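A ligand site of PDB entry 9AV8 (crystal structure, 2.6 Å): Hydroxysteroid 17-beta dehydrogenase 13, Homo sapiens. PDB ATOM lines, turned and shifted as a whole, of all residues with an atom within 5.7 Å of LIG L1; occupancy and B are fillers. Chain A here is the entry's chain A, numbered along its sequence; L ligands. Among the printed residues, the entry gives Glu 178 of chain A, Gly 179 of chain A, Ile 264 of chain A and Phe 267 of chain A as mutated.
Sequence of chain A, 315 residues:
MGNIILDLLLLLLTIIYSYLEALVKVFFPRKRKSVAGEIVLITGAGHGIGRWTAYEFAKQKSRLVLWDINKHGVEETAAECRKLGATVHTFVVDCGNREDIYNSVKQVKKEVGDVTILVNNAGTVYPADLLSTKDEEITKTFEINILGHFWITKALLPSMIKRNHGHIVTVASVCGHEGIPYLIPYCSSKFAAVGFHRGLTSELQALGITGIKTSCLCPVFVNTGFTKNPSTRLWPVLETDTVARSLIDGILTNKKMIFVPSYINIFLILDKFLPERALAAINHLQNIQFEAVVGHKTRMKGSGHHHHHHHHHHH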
ATOM      1  N   VAL A 125      10.877  -6.502 -30.683  1.00  0.00           N
ATOM      2  CA  VAL A 125      10.423  -6.688 -29.311  1.00  0.00           C
ATOM      3  C   VAL A 125      11.003  -5.613 -28.406  1.00  0.00           C
ATOM      4  O   VAL A 125      12.158  -5.225 -28.547  1.00  0.00           O
ATOM      5  CB  VAL A 125      10.725  -8.118 -28.785  1.00  0.00           C
ATOM      6  CG1 VAL A 125      12.182  -8.261 -28.371  1.00  0.00           C
ATOM      7  CG2 VAL A 125       9.814  -8.470 -27.621  1.00  0.00           C
ATOM      8  N   PRO A 127      10.853  -5.552 -24.543  1.00  0.00           N
ATOM      9  CA  PRO A 127      10.429  -6.097 -23.244  1.00  0.00           C
ATOM     10  C   PRO A 127      10.311  -5.112 -22.084  1.00  0.00           C
ATOM     11  O   PRO A 127      11.339  -4.647 -21.595  1.00  0.00           O
ATOM     12  CB  PRO A 127      11.486  -7.184 -22.944  1.00  0.00           C
ATOM     13  CG  PRO A 127      12.114  -7.500 -24.262  1.00  0.00           C
ATOM     14  CD  PRO A 127      12.077  -6.220 -25.031  1.00  0.00           C
ATOM     15  N   SER A 173       4.788 -16.528 -32.359  1.00  0.00           N
ATOM     16  CA  SER A 173       5.410 -17.241 -31.241  1.00  0.00           C
ATOM     17  C   SER A 173       4.310 -17.899 -30.389  1.00  0.00           C
ATOM     18  O   SER A 173       3.130 -17.718 -30.677  1.00  0.00           O
ATOM     19  CB  SER A 173       6.202 -16.236 -30.390  1.00  0.00           C
ATOM     20  OG  SER A 173       6.584 -16.677 -29.096  1.00  0.00           O
ATOM     21  N   VAL A 174       4.698 -18.635 -29.323  1.00  0.00           N
ATOM     22  CA  VAL A 174       3.728 -19.158 -28.349  1.00  0.00           C
ATOM     23  C   VAL A 174       2.908 -17.992 -27.714  1.00  0.00           C
ATOM     24  O   VAL A 174       1.794 -18.216 -27.240  1.00  0.00           O
ATOM     25  CB  VAL A 174       4.366 -20.057 -27.269  1.00  0.00           C
ATOM     26  CG1 VAL A 174       4.460 -21.486 -27.755  1.00  0.00           C
ATOM     27  CG2 VAL A 174       5.732 -19.538 -26.815  1.00  0.00           C
ATOM     28  N   CYS A 175       3.454 -16.747 -27.791  1.00  0.00           N
ATOM     29  CA  CYS A 175       2.879 -15.458 -27.391  1.00  0.00           C
ATOM     30  C   CYS A 175       1.696 -15.018 -28.320  1.00  0.00           C
ATOM     31  O   CYS A 175       1.278 -13.864 -28.263  1.00  0.00           O
ATOM     32  CB  CYS A 175       3.966 -14.384 -27.343  1.00  0.00           C
ATOM     33  SG  CYS A 175       5.333 -14.758 -26.222  1.00  0.00           S
ATOM     34  N   GLU A 178      -0.906 -17.659 -25.980  1.00  0.00           N
ATOM     35  CA  GLU A 178      -1.034 -17.292 -24.564  1.00  0.00           C
ATOM     36  C   GLU A 178      -0.017 -16.200 -24.137  1.00  0.00           C
ATOM     37  O   GLU A 178       1.170 -16.329 -24.423  1.00  0.00           O
ATOM     38  CB  GLU A 178      -0.981 -18.545 -23.663  1.00  0.00           C
ATOM     39  CG  GLU A 178      -0.790 -18.279 -22.192  1.00  0.00           C
ATOM     40  CD  GLU A 178       0.603 -18.642 -21.709  1.00  0.00           C
ATOM     41  OE1 GLU A 178       1.524 -18.746 -22.555  1.00  0.00           O
ATOM     42  OE2 GLU A 178       0.768 -18.838 -20.482  1.00  0.00           O
ATOM     43  N   GLY A 179      -0.508 -15.147 -23.485  1.00  0.00           N
ATOM     44  CA  GLY A 179       0.284 -13.991 -23.077  1.00  0.00           C
ATOM     45  C   GLY A 179       1.244 -14.155 -21.921  1.00  0.00           C
ATOM     46  O   GLY A 179       0.947 -14.825 -20.932  1.00  0.00           O
ATOM     47  N   ILE A 180       2.397 -13.467 -22.005  1.00  0.00           N
ATOM     48  CA  ILE A 180       3.442 -13.524 -20.987  1.00  0.00           C
ATOM     49  C   ILE A 180       3.735 -12.131 -20.358  1.00  0.00           C
ATOM     50  O   ILE A 180       3.523 -11.119 -21.025  1.00  0.00           O
ATOM     51  CB  ILE A 180       4.715 -14.222 -21.576  1.00  0.00           C
ATOM     52  CG1 ILE A 180       5.545 -13.289 -22.455  1.00  0.00           C
ATOM     53  CG2 ILE A 180       4.446 -15.547 -22.264  1.00  0.00           C
ATOM     54  CD1 ILE A 180       6.840 -13.118 -21.893  1.00  0.00           C
ATOM     55  N   LEU A 183       5.916  -8.704 -21.971  1.00  0.00           N
ATOM     56  CA  LEU A 183       5.720  -8.721 -23.415  1.00  0.00           C
ATOM     57  C   LEU A 183       4.236  -8.550 -23.806  1.00  0.00           C
ATOM     58  O   LEU A 183       3.774  -9.240 -24.684  1.00  0.00           O
ATOM     59  CB  LEU A 183       6.308 -10.012 -24.015  1.00  0.00           C
ATOM     60  CG  LEU A 183       7.796 -10.200 -23.793  1.00  0.00           C
ATOM     61  CD1 LEU A 183       8.275 -11.513 -24.374  1.00  0.00           C
ATOM     62  CD2 LEU A 183       8.593  -9.078 -24.411  1.00  0.00           C
ATOM     63  N   TYR A 186       4.051  -6.992 -27.391  1.00  0.00           N
ATOM     64  CA  TYR A 186       4.572  -8.030 -28.273  1.00  0.00           C
ATOM     65  C   TYR A 186       3.592  -9.199 -28.401  1.00  0.00           C
ATOM     66  O   TYR A 186       3.369  -9.675 -29.499  1.00  0.00           O
ATOM     67  CB  TYR A 186       5.932  -8.495 -27.773  1.00  0.00           C
ATOM     68  CG  TYR A 186       6.486  -9.709 -28.490  1.00  0.00           C
ATOM     69  CD1 TYR A 186       7.136  -9.582 -29.699  1.00  0.00           C
ATOM     70  CD2 TYR A 186       6.390 -10.974 -27.925  1.00  0.00           C
ATOM     71  CE1 TYR A 186       7.687 -10.683 -30.340  1.00  0.00           C
ATOM     72  CE2 TYR A 186       6.912 -12.084 -28.569  1.00  0.00           C
ATOM     73  CZ  TYR A 186       7.570 -11.943 -29.772  1.00  0.00           C
ATOM     74  OH  TYR A 186       8.104 -13.038 -30.386  1.00  0.00           O
ATOM     75  N   PRO A 219       7.153 -21.032 -32.240  1.00  0.00           N
ATOM     76  CA  PRO A 219       8.116 -21.649 -31.326  1.00  0.00           C
ATOM     77  C   PRO A 219       8.165 -20.996 -29.939  1.00  0.00           C
ATOM     78  O   PRO A 219       7.521 -19.975 -29.720  1.00  0.00           O
ATOM     79  CB  PRO A 219       9.441 -21.506 -32.076  1.00  0.00           C
ATOM     80  CG  PRO A 219       9.240 -20.348 -33.034  1.00  0.00           C
ATOM     81  CD  PRO A 219       7.782 -19.969 -33.038  1.00  0.00           C
ATOM     82  N   VAL A 220       8.913 -21.603 -28.995  1.00  0.00           N
ATOM     83  CA  VAL A 220       9.098 -21.046 -27.644  1.00  0.00           C
ATOM     84  C   VAL A 220      10.390 -20.145 -27.649  1.00  0.00           C
ATOM     85  O   VAL A 220      10.579 -19.472 -28.658  1.00  0.00           O
ATOM     86  CB  VAL A 220       9.012 -22.146 -26.549  1.00  0.00           C
ATOM     87  CG1 VAL A 220       7.629 -22.758 -26.505  1.00  0.00           C
ATOM     88  CG2 VAL A 220      10.070 -23.225 -26.760  1.00  0.00           C
ATOM     89  N   PHE A 221      11.256 -20.097 -26.590  1.00  0.00           N
ATOM     90  CA  PHE A 221      12.443 -19.255 -26.661  1.00  0.00           C
ATOM     91  C   PHE A 221      13.443 -19.817 -27.639  1.00  0.00           C
ATOM     92  O   PHE A 221      13.835 -20.972 -27.521  1.00  0.00           O
ATOM     93  CB  PHE A 221      13.122 -19.026 -25.307  1.00  0.00           C
ATOM     94  CG  PHE A 221      14.048 -17.831 -25.367  1.00  0.00           C
ATOM     95  CD1 PHE A 221      15.401 -17.993 -25.573  1.00  0.00           C
ATOM     96  CD2 PHE A 221      13.544 -16.539 -25.311  1.00  0.00           C
ATOM     97  CE1 PHE A 221      16.247 -16.891 -25.671  1.00  0.00           C
ATOM     98  CE2 PHE A 221      14.395 -15.440 -25.393  1.00  0.00           C
ATOM     99  CZ  PHE A 221      15.733 -15.624 -25.578  1.00  0.00           C
ATOM    100  N   PHE A 226      17.223 -12.015 -29.788  1.00  0.00           N
ATOM    101  CA  PHE A 226      15.999 -11.234 -29.972  1.00  0.00           C
ATOM    102  C   PHE A 226      15.680 -10.558 -28.607  1.00  0.00           C
ATOM    103  O   PHE A 226      15.539  -9.346 -28.508  1.00  0.00           O
ATOM    104  CB  PHE A 226      14.881 -12.175 -30.460  1.00  0.00           C
ATOM    105  CG  PHE A 226      13.581 -11.560 -30.889  1.00  0.00           C
ATOM    106  CD1 PHE A 226      13.543 -10.611 -31.891  1.00  0.00           C
ATOM    107  CD2 PHE A 226      12.385 -11.996 -30.358  1.00  0.00           C
ATOM    108  CE1 PHE A 226      12.335 -10.072 -32.308  1.00  0.00           C
ATOM    109  CE2 PHE A 226      11.179 -11.448 -30.780  1.00  0.00           C
ATOM    110  CZ  PHE A 226      11.161 -10.492 -31.744  1.00  0.00           C
ATOM    111  N   THR A 227      15.707 -11.364 -27.540  1.00  0.00           N
ATOM    112  CA  THR A 227      15.639 -10.865 -26.164  1.00  0.00           C
ATOM    113  C   THR A 227      16.909 -11.452 -25.434  1.00  0.00           C
ATOM    114  O   THR A 227      17.755 -12.082 -26.100  1.00  0.00           O
ATOM    115  CB  THR A 227      14.239 -11.080 -25.475  1.00  0.00           C
ATOM    116  OG1 THR A 227      14.297 -12.159 -24.534  1.00  0.00           O
ATOM    117  CG2 THR A 227      13.065 -11.271 -26.449  1.00  0.00           C
ATOM    118  N   ASN A 229      16.959 -13.417 -22.000  1.00  0.00           N
ATOM    119  CA  ASN A 229      16.640 -14.721 -21.413  1.00  0.00           C
ATOM    120  C   ASN A 229      15.144 -15.063 -21.590  1.00  0.00           C
ATOM    121  O   ASN A 229      14.307 -14.164 -21.725  1.00  0.00           O
ATOM    122  CB  ASN A 229      17.028 -14.730 -19.911  1.00  0.00           C
ATOM    123  CG  ASN A 229      18.462 -14.349 -19.619  1.00  0.00           C
ATOM    124  OD1 ASN A 229      19.408 -14.832 -20.250  1.00  0.00           O
ATOM    125  ND2 ASN A 229      18.641 -13.477 -18.631  1.00  0.00           N
ATOM    126  N   PRO A 230      14.777 -16.368 -21.558  1.00  0.00           N
ATOM    127  CA  PRO A 230      13.351 -16.738 -21.687  1.00  0.00           C
ATOM    128  C   PRO A 230      12.476 -16.317 -20.503  1.00  0.00           C
ATOM    129  O   PRO A 230      12.988 -16.037 -19.421  1.00  0.00           O
ATOM    130  CB  PRO A 230      13.390 -18.270 -21.799  1.00  0.00           C
ATOM    131  CG  PRO A 230      14.666 -18.671 -21.146  1.00  0.00           C
ATOM    132  CD  PRO A 230      15.643 -17.563 -21.427  1.00  0.00           C
ATOM    133  N   SER A 231      11.161 -16.309 -20.698  1.00  0.00           N
ATOM    134  CA  SER A 231      10.226 -15.915 -19.636  1.00  0.00           C
ATOM    135  C   SER A 231       9.946 -17.007 -18.589  1.00  0.00           C
ATOM    136  O   SER A 231       9.689 -16.664 -17.424  1.00  0.00           O
ATOM    137  CB  SER A 231       8.922 -15.407 -20.230  1.00  0.00           C
ATOM    138  OG  SER A 231       8.275 -16.434 -20.966  1.00  0.00           O
ATOM    139  N   THR A 232       9.965 -18.303 -18.960  1.00  0.00           N
ATOM    140  CA  THR A 232       9.635 -19.370 -18.003  1.00  0.00           C
ATOM    141  C   THR A 232      10.580 -20.595 -18.048  1.00  0.00           C
ATOM    142  O   THR A 232      11.230 -20.866 -19.061  1.00  0.00           O
ATOM    143  CB  THR A 232       8.150 -19.847 -18.130  1.00  0.00           C
ATOM    144  OG1 THR A 232       7.353 -18.980 -18.958  1.00  0.00           O
ATOM    145  CG2 THR A 232       7.479 -20.016 -16.757  1.00  0.00           C
ATOM    146  N   ARG A 233      10.642 -21.346 -16.920  1.00  0.00           N
ATOM    147  CA  ARG A 233      11.460 -22.544 -16.764  1.00  0.00           C
ATOM    148  C   ARG A 233      10.678 -23.812 -17.162  1.00  0.00           C
ATOM    149  O   ARG A 233      10.518 -24.740 -16.350  1.00  0.00           O
ATOM    150  CB  ARG A 233      11.989 -22.659 -15.315  1.00  0.00           C
ATOM    151  CG  ARG A 233      13.305 -21.915 -15.085  1.00  0.00           C
ATOM    152  CD  ARG A 233      13.800 -22.086 -13.659  1.00  0.00           C
ATOM    153  NE  ARG A 233      15.150 -21.559 -13.455  1.00  0.00           N
ATOM    154  CZ  ARG A 233      15.730 -21.423 -12.265  1.00  0.00           C
ATOM    155  NH1 ARG A 233      15.093 -21.773 -11.158  1.00  0.00           N
ATOM    156  NH2 ARG A 233      16.967 -20.937 -12.177  1.00  0.00           N
ATOM    157  N   PRO A 236      12.304 -25.018 -22.608  1.00  0.00           N
ATOM    158  CA  PRO A 236      13.494 -25.263 -23.437  1.00  0.00           C
ATOM    159  C   PRO A 236      13.920 -24.052 -24.263  1.00  0.00           C
ATOM    160  O   PRO A 236      13.094 -23.226 -24.664  1.00  0.00           O
ATOM    161  CB  PRO A 236      13.046 -26.401 -24.363  1.00  0.00           C
ATOM    162  CG  PRO A 236      11.579 -26.152 -24.555  1.00  0.00           C
ATOM    163  CD  PRO A 236      11.084 -25.596 -23.215  1.00  0.00           C
ATOM    164  N   ILE A 264       4.133 -28.478 -27.188  1.00  0.00           N
ATOM    165  CA  ILE A 264       3.481 -27.282 -26.645  1.00  0.00           C
ATOM    166  C   ILE A 264       1.973 -27.188 -27.056  1.00  0.00           C
ATOM    167  O   ILE A 264       1.267 -26.298 -26.593  1.00  0.00           O
ATOM    168  CB  ILE A 264       4.282 -26.000 -26.985  1.00  0.00           C
ATOM    169  CG1 ILE A 264       4.694 -25.962 -28.460  1.00  0.00           C
ATOM    170  CG2 ILE A 264       5.529 -25.836 -26.083  1.00  0.00           C
ATOM    171  CD1 ILE A 264       5.134 -24.700 -28.915  1.00  0.00           C
ATOM    172  N   PHE A 267       0.045 -28.688 -24.018  1.00  0.00           N
ATOM    173  CA  PHE A 267       0.047 -27.729 -22.916  1.00  0.00           C
ATOM    174  C   PHE A 267      -1.064 -26.709 -23.082  1.00  0.00           C
ATOM    175  O   PHE A 267      -1.671 -26.313 -22.084  1.00  0.00           O
ATOM    176  CB  PHE A 267       1.406 -27.034 -22.801  1.00  0.00           C
ATOM    177  CG  PHE A 267       2.457 -27.919 -22.191  1.00  0.00           C
ATOM    178  CD1 PHE A 267       2.158 -28.716 -21.101  1.00  0.00           C
ATOM    179  CD2 PHE A 267       3.741 -27.942 -22.695  1.00  0.00           C
ATOM    180  CE1 PHE A 267       3.125 -29.533 -20.533  1.00  0.00           C
ATOM    181  CE2 PHE A 267       4.709 -28.759 -22.127  1.00  0.00           C
ATOM    182  CZ  PHE A 267       4.389 -29.535 -21.044  1.00  0.00           C
ATOM    183  N   LEU A 268      -1.346 -26.294 -24.319  1.00  0.00           N
ATOM    184  CA  LEU A 268      -2.427 -25.362 -24.591  1.00  0.00           C
ATOM    185  C   LEU A 268      -3.807 -25.995 -24.401  1.00  0.00           C
ATOM    186  O   LEU A 268      -4.770 -25.292 -24.078  1.00  0.00           O
ATOM    187  CB  LEU A 268      -2.294 -24.810 -26.001  1.00  0.00           C
ATOM    188  CG  LEU A 268      -1.083 -23.933 -26.208  1.00  0.00           C
ATOM    189  CD1 LEU A 268      -0.856 -23.666 -27.669  1.00  0.00           C
ATOM    190  CD2 LEU A 268      -1.202 -22.630 -25.423  1.00  0.00           C
ATOM    191  N   ASP A 271      -4.703 -25.837 -20.735  1.00  0.00           N
ATOM    192  CA  ASP A 271      -5.031 -24.465 -20.341  1.00  0.00           C
ATOM    193  C   ASP A 271      -6.555 -24.244 -20.352  1.00  0.00           C
ATOM    194  O   ASP A 271      -7.060 -23.471 -19.544  1.00  0.00           O
ATOM    195  CB  ASP A 271      -4.345 -23.439 -21.269  1.00  0.00           C
ATOM    196  CG  ASP A 271      -2.910 -23.105 -20.899  1.00  0.00           C
ATOM    197  OD1 ASP A 271      -2.489 -23.446 -19.765  1.00  0.00           O
ATOM    198  OD2 ASP A 271      -2.206 -22.493 -21.738  1.00  0.00           O
HETATM  199  C1  LIG L   1      10.164 -14.916 -25.413  1.00  0.00           C
HETATM  200  N1  LIG L   1      11.017 -13.845 -23.669  1.00  0.00           N
HETATM  201  C2  LIG L   1       8.973 -17.456 -25.510  1.00  0.00           C
HETATM  202  C3  LIG L   1       8.980 -16.650 -26.628  1.00  0.00           C
HETATM  203  C4  LIG L   1      10.147 -15.724 -24.260  1.00  0.00           C
HETATM  204  C5  LIG L   1       6.855 -19.129 -23.216  1.00  0.00           C
HETATM  205  C6  LIG L   1       9.545 -17.006 -24.321  1.00  0.00           C
HETATM  206  C7  LIG L   1       5.321 -20.992 -23.100  1.00  0.00           C
HETATM  207  C8  LIG L   1       7.689 -21.354 -22.825  1.00  0.00           C
HETATM  208  C9  LIG L   1       5.569 -19.626 -23.274  1.00  0.00           C
HETATM  209  C10 LIG L   1       1.094 -22.144 -21.454  1.00  0.00           C
HETATM  210  C11 LIG L   1      11.492 -12.811 -22.756  1.00  0.00           C
HETATM  211  C12 LIG L   1      10.759 -13.682 -24.974  1.00  0.00           C
HETATM  212  C13 LIG L   1       9.570 -15.383 -26.597  1.00  0.00           C
HETATM  213  N2  LIG L   1      10.683 -15.082 -23.187  1.00  0.00           N
HETATM  214  N3  LIG L   1       9.450 -17.748 -23.110  1.00  0.00           N
HETATM  215  S1  LIG L   1       9.551 -19.369 -22.899  1.00  0.00           S
HETATM  216  O1  LIG L   1      10.301 -19.919 -23.990  1.00  0.00           O
HETATM  217  O2  LIG L   1      10.029 -19.555 -21.565  1.00  0.00           O
HETATM  218  C14 LIG L   1       7.904 -20.002 -22.988  1.00  0.00           C
HETATM  219  C15 LIG L   1       6.392 -21.847 -22.877  1.00  0.00           C
HETATM  220 CL1  LIG L   1       4.253 -18.541 -23.574  1.00  0.00          CL
HETATM  221  C16 LIG L   1       9.574 -14.621 -27.894  1.00  0.00           C
HETATM  222  O3  LIG L   1       8.840 -14.957 -28.800  1.00  0.00           O
HETATM  223  O4  LIG L   1      10.313 -13.557 -27.938  1.00  0.00           O
HETATM  224  O5  LIG L   1       4.010 -21.391 -23.153  1.00  0.00           O
HETATM  225  C17 LIG L   1       3.718 -22.782 -22.891  1.00  0.00           C
HETATM  226  C18 LIG L   1       2.236 -23.002 -23.055  1.00  0.00           C
HETATM  227  C19 LIG L   1       1.322 -21.771 -22.933  1.00  0.00           C
HETATM  228  C20 LIG L   1       1.580 -23.555 -21.780  1.00  0.00           C
HETATM  229  P1  LG2 L   2      16.493 -11.784 -34.730  1.00  0.00           P
HETATM  230  O1  LG2 L   2      17.605 -12.761 -34.650  1.00  0.00           O
HETATM  231  O2  LG2 L   2      16.533 -10.587 -33.871  1.00  0.00           O
HETATM  232  O3  LG2 L   2      16.372 -11.363 -36.263  1.00  0.00           O
HETATM  233  C1  LG2 L   2      15.170 -10.726 -36.751  1.00  0.00           C
HETATM  234  C2  LG2 L   2      15.506  -9.972 -38.009  1.00  0.00           C
HETATM  235  O4  LG2 L   2      14.405  -9.104 -38.357  1.00  0.00           O
HETATM  236  C3  LG2 L   2      16.768  -9.093 -37.938  1.00  0.00           C
HETATM  237  O5  LG2 L   2      17.769  -9.529 -38.859  1.00  0.00           O
HETATM  238  C4  LG2 L   2      16.248  -7.674 -38.229  1.00  0.00           C
HETATM  239  O6  LG2 L   2      17.142  -6.895 -39.019  1.00  0.00           O
HETATM  240  C5  LG2 L   2      14.940  -7.943 -38.964  1.00  0.00           C
HETATM  241  N1  LG2 L   2      13.971  -6.852 -38.856  1.00  0.00           N
HETATM  242  C6  LG2 L   2      13.527  -6.243 -37.714  1.00  0.00           C
HETATM  243  N2  LG2 L   2      12.749  -5.210 -37.926  1.00  0.00           N
HETATM  244  C7  LG2 L   2      12.669  -5.137 -39.308  1.00  0.00           C
HETATM  245  C8  LG2 L   2      12.016  -4.240 -40.173  1.00  0.00           C
HETATM  246  N3  LG2 L   2      11.321  -3.175 -39.767  1.00  0.00           N
HETATM  247  N4  LG2 L   2      12.158  -4.444 -41.503  1.00  0.00           N
HETATM  248  C9  LG2 L   2      12.898  -5.465 -41.924  1.00  0.00           C
HETATM  249  N5  LG2 L   2      13.568  -6.376 -41.202  1.00  0.00           N
HETATM  250  C10 LG2 L   2      13.410  -6.147 -39.891  1.00  0.00           C
HETATM  251  O7  LG2 L   2      15.107 -12.558 -34.503  1.00  0.00           O
HETATM  252  P2  LG2 L   2      14.634 -14.082 -34.633  1.00  0.00           P
HETATM  253  O8  LG2 L   2      14.926 -14.578 -35.995  1.00  0.00           O
HETATM  254  O9  LG2 L   2      15.117 -14.835 -33.457  1.00  0.00           O
HETATM  255  O10 LG2 L   2      13.045 -13.917 -34.555  1.00  0.00           O
HETATM  256  C11 LG2 L   2      12.384 -13.010 -35.465  1.00  0.00           C
HETATM  257  C12 LG2 L   2      10.948 -13.423 -35.630  1.00  0.00           C
HETATM  258  O11 LG2 L   2      10.749 -14.721 -35.025  1.00  0.00           O
HETATM  259  C13 LG2 L   2       9.914 -12.482 -34.990  1.00  0.00           C
HETATM  260  O12 LG2 L   2       8.762 -12.344 -35.810  1.00  0.00           O
HETATM  261  C14 LG2 L   2       9.618 -13.171 -33.651  1.00  0.00           C
HETATM  262  O13 LG2 L   2       8.332 -12.838 -33.133  1.00  0.00           O
HETATM  263  C15 LG2 L   2       9.749 -14.651 -34.035  1.00  0.00           C
HETATM  264  N6  LG2 L   2      10.144 -15.514 -32.866  1.00  0.00           N
HETATM  265  C16 LG2 L   2      11.338 -15.314 -32.277  1.00  0.00           C
HETATM  266  C17 LG2 L   2      11.686 -16.027 -31.140  1.00  0.00           C
HETATM  267  C18 LG2 L   2      13.029 -15.844 -30.487  1.00  0.00           C
HETATM  268  O14 LG2 L   2      13.139 -15.973 -29.256  1.00  0.00           O
HETATM  269  N7  LG2 L   2      14.061 -15.541 -31.285  1.00  0.00           N
HETATM  270  C19 LG2 L   2      10.768 -16.943 -30.634  1.00  0.00           C
HETATM  271  C20 LG2 L   2       9.557 -17.146 -31.274  1.00  0.00           C
HETATM  272  C21 LG2 L   2       9.256 -16.418 -32.395  1.00  0.00           C
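CG2 of Val 174 touches C9 of LIG L1, at 3.5 Å.
OE1 of Glu 178 touches CL1 of LIG L1 (2.9 Å).
Ile 180 touches LIG L1 (CG2 to CL1, 3.3 Å).
Leu 183 touches LIG L1.
CB of Val 220 touches O1 of LIG L1, 3.6 Å away.
CD2 of Phe 226 touches O4 of LIG L1 (3.5 Å).
OG1 of Thr 227 touches C11 of LIG L1 (3.4 Å).
Asn 229 touches LIG L1 (O to C11, 3.3 Å).
Pro 230 touches LIG L1.
Phe 267 touches LIG L1 (CB to C20, 3.6 Å).
CD2 of Leu 268 touches C19 of LIG L1 (3.6 Å).
Asp 271 touches LIG L1 (OD2 to C10, 3.3 Å).
Hydrophobic or aromatic side chains within 4 Å of LIG L1: Val 174, Ile 180, Leu 183, Tyr 186, Val 220, Phe 221, Phe 226, Pro 230, Phe 267 and Leu 268.
17 residues have an atom within 4 Å of LIG L1: Ser 173, Val 174, Glu 178, Ile 180, Leu 183, Tyr 186, Val 220, Phe 221, Phe 226, Thr 227, Asn 229, Pro 230, Ser 231, Thr 232, Phe 267, Leu 268 and Asp 271.
The nearest printed residue that does not touch LIG L1 is Cys 175 (4.1 Å).
The side-chain hydroxyl of Tyr 186 sits at hydrogen-bond distance from an oxygen (O3) of LIG L1.
N of Phe 221 is in hydrogen-bond range of O1 of LIG L1 (2.8 Å).
N2 of LIG L1 lies within hydrogen-bond range of N of Ser 231, at 2.8 Å.
OG of Ser 231 sits at hydrogen-bond distance from N3 of LIG L1, at 2.8 Å.
An oxygen (O3) of LIG L1 lies within hydrogen-bond range of the side-chain hydroxyl (OG) of Ser 173, 2.9 Å away.
N of Thr 232 lies within hydrogen-bond range of O2 of LIG L1, 2.9 Å away.
O13 of LG2 L2 sits at hydrogen-bond distance from OH of Tyr 186.
OG of Ser 231 lies close to OG1 of Thr 232 (3.4 Å).
The side-chain hydroxyl (OG) of Ser 173 lies close to the backbone NH (N) of Cys 175, 3.4 Å away.
OG of Ser 173 lies within hydrogen-bond range of O of Pro 219 (3.5 Å).
The side-chain hydroxyl of Thr 227 is in hydrogen-bond range of the backbone carbonyl oxygen of Asn 229.
N of Val 174 sits at hydrogen-bond distance from O of Pro 219 (3.2 Å).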
